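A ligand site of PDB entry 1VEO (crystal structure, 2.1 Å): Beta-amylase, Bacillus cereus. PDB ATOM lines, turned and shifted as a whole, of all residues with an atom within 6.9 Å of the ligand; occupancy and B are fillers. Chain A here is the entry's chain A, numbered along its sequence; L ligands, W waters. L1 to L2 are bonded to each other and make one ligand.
O2 of LIG L1 sits at hydrogen-bond distance from NE2 of Gln 239 (2.7 Å).
The backbone carbonyl oxygen (O) of Ala 230 lies within hydrogen-bond range of an oxygen (O3) of LG2 L2, 2.7 Å away.
An oxygen (O1) of LG2 L2 sits at hydrogen-bond distance from the backbone NH (N) of Ser 235.
An oxygen (O1) of LG2 L2 lies within hydrogen-bond range of the side-chain hydroxyl of Ser 235 (2.7 Å).
O5 of LG2 L2 sits at hydrogen-bond distance from N of Leu 232, 2.8 Å away.
An oxygen (O5) of LG2 L2 lies within hydrogen-bond range of the backbone carbonyl oxygen (O) of Leu 232 (3.3 Å).
The side-chain hydroxyl of Tyr 249 sits close to an oxygen (O4) of LG2 L2, 3.2 Å away.
The backbone carbonyl oxygen (O) of Gln 239 lies within hydrogen-bond range of the backbone NH (N) of Gly 244.
OD1 of Asp 236 lies within hydrogen-bond range of N of Gln 239 (2.9 Å).
The side-chain amide nitrogen of Asn 243 lies within hydrogen-bond range of the side-chain amide oxygen of Gln 239 (3.1 Å).
The backbone carbonyl oxygen of Leu 232 sits at hydrogen-bond distance from the side-chain hydroxyl of Tyr 249, 2.4 Å away.
The side-chain hydroxyl (OG) of Ser 247 sits close to the backbone NH (N) of Tyr 249 (3.5 Å).
O of Gly 244 lies within hydrogen-bond range of OG of Ser 247 (2.9 Å).
The backbone carbonyl oxygen (O) of Phe 240 is in hydrogen-bond range of the backbone NH (N) of Tyr 245.
Merely in contact with the ligand: Gly 244 (3.1 Å), Ile 231 (3.4 Å), Phe 240 (3.4 Å), Pro 233 (3.5 Å), Thr 223 (3.6 Å), Pro 234 (3.6 Å) and Trp 221 (3.7 Å).
Hydrophobic or aromatic side chains that line the ligand: Trp 221, Pro 234, Phe 240 and Tyr 249.
Within 4 Å of the ligand: Trp 221, Thr 223, Ala 230, Ile 231, Leu 232, Pro 233, Pro 234, Ser 235, Gln 239, Phe 240, Gly 244 and Tyr 249.
The nearest printed residue that does not touch the ligand is Ser 247 (4.1 Å).
Water W2 lies within hydrogen-bond range of O6 of LIG L1 and OG of Ser 247.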
ATOM      1  N   PHE A 203       7.193  -2.808 -32.808  1.00  0.00           N
ATOM      2  CA  PHE A 203       6.883  -3.967 -31.988  1.00  0.00           C
ATOM      3  C   PHE A 203       6.887  -5.208 -32.880  1.00  0.00           C
ATOM      4  O   PHE A 203       7.411  -6.253 -32.503  1.00  0.00           O
ATOM      5  CB  PHE A 203       5.520  -3.824 -31.304  1.00  0.00           C
ATOM      6  CG  PHE A 203       5.097  -5.040 -30.531  1.00  0.00           C
ATOM      7  CD1 PHE A 203       5.895  -5.547 -29.512  1.00  0.00           C
ATOM      8  CD2 PHE A 203       3.916  -5.704 -30.855  1.00  0.00           C
ATOM      9  CE1 PHE A 203       5.508  -6.694 -28.814  1.00  0.00           C
ATOM     10  CE2 PHE A 203       3.522  -6.847 -30.163  1.00  0.00           C
ATOM     11  CZ  PHE A 203       4.329  -7.349 -29.152  1.00  0.00           C
ATOM     12  N   VAL A 217       6.742 -17.409 -33.869  1.00  0.00           N
ATOM     13  CA  VAL A 217       5.957 -16.522 -33.026  1.00  0.00           C
ATOM     14  C   VAL A 217       4.720 -17.297 -32.582  1.00  0.00           C
ATOM     15  O   VAL A 217       4.483 -17.477 -31.389  1.00  0.00           O
ATOM     16  CB  VAL A 217       5.515 -15.254 -33.794  1.00  0.00           C
ATOM     17  CG1 VAL A 217       4.550 -14.431 -32.950  1.00  0.00           C
ATOM     18  CG2 VAL A 217       6.741 -14.425 -34.154  1.00  0.00           C
ATOM     19  N   TRP A 221       3.784 -17.959 -28.695  1.00  0.00           N
ATOM     20  CA  TRP A 221       2.581 -17.373 -28.116  1.00  0.00           C
ATOM     21  C   TRP A 221       1.408 -18.354 -28.085  1.00  0.00           C
ATOM     22  O   TRP A 221       0.362 -18.052 -27.522  1.00  0.00           O
ATOM     23  CB  TRP A 221       2.171 -16.121 -28.884  1.00  0.00           C
ATOM     24  CG  TRP A 221       3.136 -14.960 -28.773  1.00  0.00           C
ATOM     25  CD1 TRP A 221       4.218 -14.866 -27.937  1.00  0.00           C
ATOM     26  CD2 TRP A 221       3.078 -13.719 -29.499  1.00  0.00           C
ATOM     27  NE1 TRP A 221       4.837 -13.649 -28.098  1.00  0.00           N
ATOM     28  CE2 TRP A 221       4.162 -12.933 -29.056  1.00  0.00           C
ATOM     29  CE3 TRP A 221       2.232 -13.209 -30.487  1.00  0.00           C
ATOM     30  CZ2 TRP A 221       4.410 -11.650 -29.555  1.00  0.00           C
ATOM     31  CZ3 TRP A 221       2.476 -11.947 -30.994  1.00  0.00           C
ATOM     32  CH2 TRP A 221       3.561 -11.170 -30.523  1.00  0.00           C
ATOM     33  N   GLY A 222       1.599 -19.533 -28.669  1.00  0.00           N
ATOM     34  CA  GLY A 222       0.524 -20.500 -28.706  1.00  0.00           C
ATOM     35  C   GLY A 222      -0.660 -19.894 -29.418  1.00  0.00           C
ATOM     36  O   GLY A 222      -1.806 -20.180 -29.101  1.00  0.00           O
ATOM     37  N   THR A 223      -0.381 -19.040 -30.394  1.00  0.00           N
ATOM     38  CA  THR A 223      -1.421 -18.375 -31.150  1.00  0.00           C
ATOM     39  C   THR A 223      -1.568 -18.950 -32.553  1.00  0.00           C
ATOM     40  O   THR A 223      -0.893 -19.920 -32.913  1.00  0.00           O
ATOM     41  CB  THR A 223      -1.123 -16.878 -31.257  1.00  0.00           C
ATOM     42  OG1 THR A 223       0.200 -16.690 -31.764  1.00  0.00           O
ATOM     43  CG2 THR A 223      -1.244 -16.211 -29.887  1.00  0.00           C
ATOM     44  N   LYS A 224      -2.421 -18.327 -33.354  1.00  0.00           N
ATOM     45  CA  LYS A 224      -2.665 -18.782 -34.710  1.00  0.00           C
ATOM     46  C   LYS A 224      -2.750 -17.581 -35.656  1.00  0.00           C
ATOM     47  O   LYS A 224      -3.642 -17.514 -36.496  1.00  0.00           O
ATOM     48  CB  LYS A 224      -3.989 -19.554 -34.755  1.00  0.00           C
ATOM     49  CG  LYS A 224      -4.101 -20.564 -35.879  1.00  0.00           C
ATOM     50  CD  LYS A 224      -3.794 -21.975 -35.396  1.00  0.00           C
ATOM     51  CE  LYS A 224      -2.333 -22.127 -34.954  1.00  0.00           C
ATOM     52  NZ  LYS A 224      -2.044 -23.518 -34.489  1.00  0.00           N
ATOM     53  N   LEU A 225      -1.821 -16.647 -35.501  1.00  0.00           N
ATOM     54  CA  LEU A 225      -1.791 -15.468 -36.347  1.00  0.00           C
ATOM     55  C   LEU A 225      -1.662 -15.861 -37.819  1.00  0.00           C
ATOM     56  O   LEU A 225      -0.818 -16.671 -38.194  1.00  0.00           O
ATOM     57  CB  LEU A 225      -0.614 -14.563 -35.951  1.00  0.00           C
ATOM     58  CG  LEU A 225      -0.757 -13.752 -34.655  1.00  0.00           C
ATOM     59  CD1 LEU A 225      -1.204 -14.649 -33.522  1.00  0.00           C
ATOM     60  CD2 LEU A 225       0.585 -13.102 -34.304  1.00  0.00           C
ATOM     61  N   LEU A 229       1.234  -9.015 -40.212  1.00  0.00           N
ATOM     62  CA  LEU A 229       0.489  -7.806 -39.855  1.00  0.00           C
ATOM     63  C   LEU A 229      -0.410  -8.017 -38.643  1.00  0.00           C
ATOM     64  O   LEU A 229      -0.885  -7.062 -38.040  1.00  0.00           O
ATOM     65  CB  LEU A 229      -0.370  -7.319 -41.038  1.00  0.00           C
ATOM     66  CG  LEU A 229       0.304  -6.654 -42.248  1.00  0.00           C
ATOM     67  CD1 LEU A 229       1.255  -5.573 -41.779  1.00  0.00           C
ATOM     68  CD2 LEU A 229       1.035  -7.704 -43.054  1.00  0.00           C
ATOM     69  N   ALA A 230      -0.653  -9.274 -38.295  1.00  0.00           N
ATOM     70  CA  ALA A 230      -1.497  -9.616 -37.150  1.00  0.00           C
ATOM     71  C   ALA A 230      -0.755  -9.419 -35.836  1.00  0.00           C
ATOM     72  O   ALA A 230      -1.349  -9.477 -34.750  1.00  0.00           O
ATOM     73  CB  ALA A 230      -1.986 -11.046 -37.263  1.00  0.00           C
ATOM     74  N   ILE A 231       0.558  -9.222 -35.916  1.00  0.00           N
ATOM     75  CA  ILE A 231       1.357  -8.979 -34.717  1.00  0.00           C
ATOM     76  C   ILE A 231       1.056  -7.527 -34.363  1.00  0.00           C
ATOM     77  O   ILE A 231       1.452  -6.611 -35.097  1.00  0.00           O
ATOM     78  CB  ILE A 231       2.865  -9.171 -34.984  1.00  0.00           C
ATOM     79  CG1 ILE A 231       3.146 -10.626 -35.385  1.00  0.00           C
ATOM     80  CG2 ILE A 231       3.665  -8.815 -33.751  1.00  0.00           C
ATOM     81  CD1 ILE A 231       4.613 -10.910 -35.693  1.00  0.00           C
ATOM     82  N   LEU A 232       0.357  -7.315 -33.250  1.00  0.00           N
ATOM     83  CA  LEU A 232      -0.049  -5.976 -32.847  1.00  0.00           C
ATOM     84  C   LEU A 232      -0.104  -5.766 -31.341  1.00  0.00           C
ATOM     85  O   LEU A 232      -0.084  -6.714 -30.556  1.00  0.00           O
ATOM     86  CB  LEU A 232      -1.443  -5.683 -33.394  1.00  0.00           C
ATOM     87  CG  LEU A 232      -1.675  -5.633 -34.904  1.00  0.00           C
ATOM     88  CD1 LEU A 232      -3.165  -5.709 -35.188  1.00  0.00           C
ATOM     89  CD2 LEU A 232      -1.083  -4.362 -35.474  1.00  0.00           C
ATOM     90  N   PRO A 233      -0.159  -4.494 -30.913  1.00  0.00           N
ATOM     91  CA  PRO A 233      -0.222  -4.192 -29.480  1.00  0.00           C
ATOM     92  C   PRO A 233      -1.637  -4.573 -29.083  1.00  0.00           C
ATOM     93  O   PRO A 233      -2.457  -4.882 -29.957  1.00  0.00           O
ATOM     94  CB  PRO A 233      -0.010  -2.678 -29.426  1.00  0.00           C
ATOM     95  CG  PRO A 233       0.765  -2.394 -30.677  1.00  0.00           C
ATOM     96  CD  PRO A 233       0.072  -3.258 -31.685  1.00  0.00           C
ATOM     97  N   PRO A 234      -1.966  -4.556 -27.782  1.00  0.00           N
ATOM     98  CA  PRO A 234      -3.315  -4.924 -27.338  1.00  0.00           C
ATOM     99  C   PRO A 234      -4.427  -4.118 -28.016  1.00  0.00           C
ATOM    100  O   PRO A 234      -4.325  -2.904 -28.154  1.00  0.00           O
ATOM    101  CB  PRO A 234      -3.265  -4.667 -25.835  1.00  0.00           C
ATOM    102  CG  PRO A 234      -1.829  -4.888 -25.493  1.00  0.00           C
ATOM    103  CD  PRO A 234      -1.109  -4.211 -26.632  1.00  0.00           C
ATOM    104  N   SER A 235      -5.478  -4.797 -28.451  1.00  0.00           N
ATOM    105  CA  SER A 235      -6.610  -4.137 -29.091  1.00  0.00           C
ATOM    106  C   SER A 235      -7.494  -3.582 -27.975  1.00  0.00           C
ATOM    107  O   SER A 235      -8.109  -2.527 -28.118  1.00  0.00           O
ATOM    108  CB  SER A 235      -7.433  -5.140 -29.911  1.00  0.00           C
ATOM    109  OG  SER A 235      -6.649  -5.719 -30.945  1.00  0.00           O
ATOM    110  N   ASP A 236      -7.542  -4.325 -26.877  1.00  0.00           N
ATOM    111  CA  ASP A 236      -8.352  -3.953 -25.727  1.00  0.00           C
ATOM    112  C   ASP A 236      -7.450  -3.853 -24.491  1.00  0.00           C
ATOM    113  O   ASP A 236      -7.109  -4.861 -23.884  1.00  0.00           O
ATOM    114  CB  ASP A 236      -9.424  -5.035 -25.504  1.00  0.00           C
ATOM    115  CG  ASP A 236     -10.369  -4.708 -24.383  1.00  0.00           C
ATOM    116  OD1 ASP A 236      -9.936  -4.027 -23.416  1.00  0.00           O
ATOM    117  OD2 ASP A 236     -11.546  -5.128 -24.448  1.00  0.00           O
ATOM    118  N   GLY A 237      -7.067  -2.630 -24.139  1.00  0.00           N
ATOM    119  CA  GLY A 237      -6.188  -2.431 -22.987  1.00  0.00           C
ATOM    120  C   GLY A 237      -6.731  -2.990 -21.687  1.00  0.00           C
ATOM    121  O   GLY A 237      -5.987  -3.534 -20.868  1.00  0.00           O
ATOM    122  N   GLN A 239      -8.930  -5.565 -21.218  1.00  0.00           N
ATOM    123  CA  GLN A 239      -8.864  -7.017 -21.226  1.00  0.00           C
ATOM    124  C   GLN A 239      -7.410  -7.456 -21.030  1.00  0.00           C
ATOM    125  O   GLN A 239      -7.143  -8.411 -20.327  1.00  0.00           O
ATOM    126  CB  GLN A 239      -9.431  -7.564 -22.535  1.00  0.00           C
ATOM    127  CG  GLN A 239      -9.460  -9.082 -22.602  1.00  0.00           C
ATOM    128  CD  GLN A 239      -8.153  -9.675 -23.128  1.00  0.00           C
ATOM    129  OE1 GLN A 239      -7.798 -10.801 -22.775  1.00  0.00           O
ATOM    130  NE2 GLN A 239      -7.464  -8.926 -23.984  1.00  0.00           N
ATOM    131  N   PHE A 240      -6.481  -6.720 -21.642  1.00  0.00           N
ATOM    132  CA  PHE A 240      -5.070  -7.048 -21.496  1.00  0.00           C
ATOM    133  C   PHE A 240      -4.632  -6.948 -20.037  1.00  0.00           C
ATOM    134  O   PHE A 240      -3.884  -7.799 -19.546  1.00  0.00           O
ATOM    135  CB  PHE A 240      -4.195  -6.124 -22.325  1.00  0.00           C
ATOM    136  CG  PHE A 240      -2.729  -6.425 -22.217  1.00  0.00           C
ATOM    137  CD1 PHE A 240      -2.163  -7.444 -22.962  1.00  0.00           C
ATOM    138  CD2 PHE A 240      -1.931  -5.711 -21.337  1.00  0.00           C
ATOM    139  CE1 PHE A 240      -0.815  -7.763 -22.833  1.00  0.00           C
ATOM    140  CE2 PHE A 240      -0.576  -6.022 -21.194  1.00  0.00           C
ATOM    141  CZ  PHE A 240      -0.014  -7.049 -21.939  1.00  0.00           C
ATOM    142  N   LEU A 241      -5.100  -5.903 -19.351  1.00  0.00           N
ATOM    143  CA  LEU A 241      -4.756  -5.678 -17.955  1.00  0.00           C
ATOM    144  C   LEU A 241      -5.461  -6.639 -17.000  1.00  0.00           C
ATOM    145  O   LEU A 241      -4.969  -6.908 -15.904  1.00  0.00           O
ATOM    146  CB  LEU A 241      -5.078  -4.236 -17.561  1.00  0.00           C
ATOM    147  CG  LEU A 241      -4.203  -3.169 -18.210  1.00  0.00           C
ATOM    148  CD1 LEU A 241      -4.742  -1.787 -17.888  1.00  0.00           C
ATOM    149  CD2 LEU A 241      -2.766  -3.307 -17.727  1.00  0.00           C
ATOM    150  N   ASN A 243      -6.197  -9.947 -17.729  1.00  0.00           N
ATOM    151  CA  ASN A 243      -5.551 -11.249 -17.749  1.00  0.00           C
ATOM    152  C   ASN A 243      -4.664 -11.528 -18.959  1.00  0.00           C
ATOM    153  O   ASN A 243      -3.892 -12.477 -18.953  1.00  0.00           O
ATOM    154  CB  ASN A 243      -6.606 -12.343 -17.609  1.00  0.00           C
ATOM    155  CG  ASN A 243      -7.745 -12.165 -18.585  1.00  0.00           C
ATOM    156  OD1 ASN A 243      -8.897 -12.413 -18.235  1.00  0.00           O
ATOM    157  ND2 ASN A 243      -7.432 -11.754 -19.800  1.00  0.00           N
ATOM    158  N   GLY A 244      -4.770 -10.702 -19.994  1.00  0.00           N
ATOM    159  CA  GLY A 244      -3.938 -10.917 -21.161  1.00  0.00           C
ATOM    160  C   GLY A 244      -2.453 -10.814 -20.817  1.00  0.00           C
ATOM    161  O   GLY A 244      -1.608 -11.476 -21.435  1.00  0.00           O
ATOM    162  N   TYR A 245      -2.152  -9.997 -19.818  1.00  0.00           N
ATOM    163  CA  TYR A 245      -0.774  -9.790 -19.390  1.00  0.00           C
ATOM    164  C   TYR A 245      -0.125 -11.073 -18.870  1.00  0.00           C
ATOM    165  O   TYR A 245       1.090 -11.180 -18.819  1.00  0.00           O
ATOM    166  CB  TYR A 245      -0.711  -8.722 -18.290  1.00  0.00           C
ATOM    167  CG  TYR A 245      -1.284  -9.152 -16.956  1.00  0.00           C
ATOM    168  CD1 TYR A 245      -2.662  -9.096 -16.698  1.00  0.00           C
ATOM    169  CD2 TYR A 245      -0.451  -9.622 -15.941  1.00  0.00           C
ATOM    170  CE1 TYR A 245      -3.178  -9.503 -15.459  1.00  0.00           C
ATOM    171  CE2 TYR A 245      -0.955 -10.023 -14.696  1.00  0.00           C
ATOM    172  CZ  TYR A 245      -2.317  -9.954 -14.470  1.00  0.00           C
ATOM    173  OH  TYR A 245      -2.803 -10.331 -13.235  1.00  0.00           O
ATOM    174  N   SER A 247      -0.226 -14.037 -20.287  1.00  0.00           N
ATOM    175  CA  SER A 247       0.212 -14.912 -21.375  1.00  0.00           C
ATOM    176  C   SER A 247       1.610 -14.596 -21.917  1.00  0.00           C
ATOM    177  O   SER A 247       2.198 -13.558 -21.600  1.00  0.00           O
ATOM    178  CB  SER A 247      -0.780 -14.828 -22.534  1.00  0.00           C
ATOM    179  OG  SER A 247      -0.724 -13.564 -23.164  1.00  0.00           O
ATOM    180  N   TYR A 249       2.351 -13.771 -24.802  1.00  0.00           N
ATOM    181  CA  TYR A 249       2.245 -12.578 -25.636  1.00  0.00           C
ATOM    182  C   TYR A 249       2.343 -11.345 -24.742  1.00  0.00           C
ATOM    183  O   TYR A 249       3.079 -10.407 -25.040  1.00  0.00           O
ATOM    184  CB  TYR A 249       0.884 -12.545 -26.341  1.00  0.00           C
ATOM    185  CG  TYR A 249       0.542 -11.173 -26.856  1.00  0.00           C
ATOM    186  CD1 TYR A 249       1.148 -10.663 -28.004  1.00  0.00           C
ATOM    187  CD2 TYR A 249      -0.344 -10.340 -26.162  1.00  0.00           C
ATOM    188  CE1 TYR A 249       0.882  -9.360 -28.450  1.00  0.00           C
ATOM    189  CE2 TYR A 249      -0.612  -9.048 -26.594  1.00  0.00           C
ATOM    190  CZ  TYR A 249       0.010  -8.568 -27.748  1.00  0.00           C
ATOM    191  OH  TYR A 249      -0.258  -7.299 -28.195  1.00  0.00           O
ATOM    192  N   GLY A 250       1.588 -11.353 -23.659  1.00  0.00           N
ATOM    193  CA  GLY A 250       1.587 -10.225 -22.739  1.00  0.00           C
ATOM    194  C   GLY A 250       2.976  -9.930 -22.215  1.00  0.00           C
ATOM    195  O   GLY A 250       3.410  -8.790 -22.180  1.00  0.00           O
HETATM  196  C1  LIG L   1      -4.372 -11.709 -24.741  1.00  0.00           C
HETATM  197  C2  LIG L   1      -4.112 -10.200 -24.753  1.00  0.00           C
HETATM  198  C3  LIG L   1      -4.500  -9.625 -26.111  1.00  0.00           C
HETATM  199  C4  LIG L   1      -3.732 -10.345 -27.216  1.00  0.00           C
HETATM  200  C5  LIG L   1      -3.972 -11.861 -27.128  1.00  0.00           C
HETATM  201  C6  LIG L   1      -3.117 -12.633 -28.114  1.00  0.00           C
HETATM  202  O1  LIG L   1      -5.720 -11.956 -24.931  1.00  0.00           O
HETATM  203  O2  LIG L   1      -4.904  -9.584 -23.737  1.00  0.00           O
HETATM  204  O3  LIG L   1      -4.190  -8.243 -26.148  1.00  0.00           O
HETATM  205  O4  LIG L   1      -4.177  -9.861 -28.503  1.00  0.00           O
HETATM  206  O5  LIG L   1      -3.638 -12.354 -25.806  1.00  0.00           O
HETATM  207  O6  LIG L   1      -3.444 -14.018 -28.111  1.00  0.00           O
HETATM  208  C1  LG2 L   2      -3.353  -8.866 -29.060  1.00  0.00           C
HETATM  209  C2  LG2 L   2      -4.146  -7.999 -30.031  1.00  0.00           C
HETATM  210  C3  LG2 L   2      -4.426  -8.739 -31.346  1.00  0.00           C
HETATM  211  C4  LG2 L   2      -3.126  -9.274 -31.933  1.00  0.00           C
HETATM  212  C5  LG2 L   2      -2.456 -10.176 -30.891  1.00  0.00           C
HETATM  213  C6  LG2 L   2      -1.128 -10.733 -31.369  1.00  0.00           C
HETATM  214  O1  LG2 L   2      -5.364  -7.607 -29.431  1.00  0.00           O
HETATM  215  O2  LG2 L   2      -5.047  -7.869 -32.277  1.00  0.00           O
HETATM  216  O3  LG2 L   2      -3.385  -9.997 -33.122  1.00  0.00           O
HETATM  217  O4  LG2 L   2      -2.193  -9.421 -29.687  1.00  0.00           O
HETATM  218  O5  LG2 L   2      -0.324  -9.693 -31.905  1.00  0.00           O
HETATM  219  O   HOH W   1      -6.450  -6.812 -25.974  1.00  0.00           O
HETATM  220  O   HOH W   2      -2.453 -14.880 -25.815  1.00  0.00           O
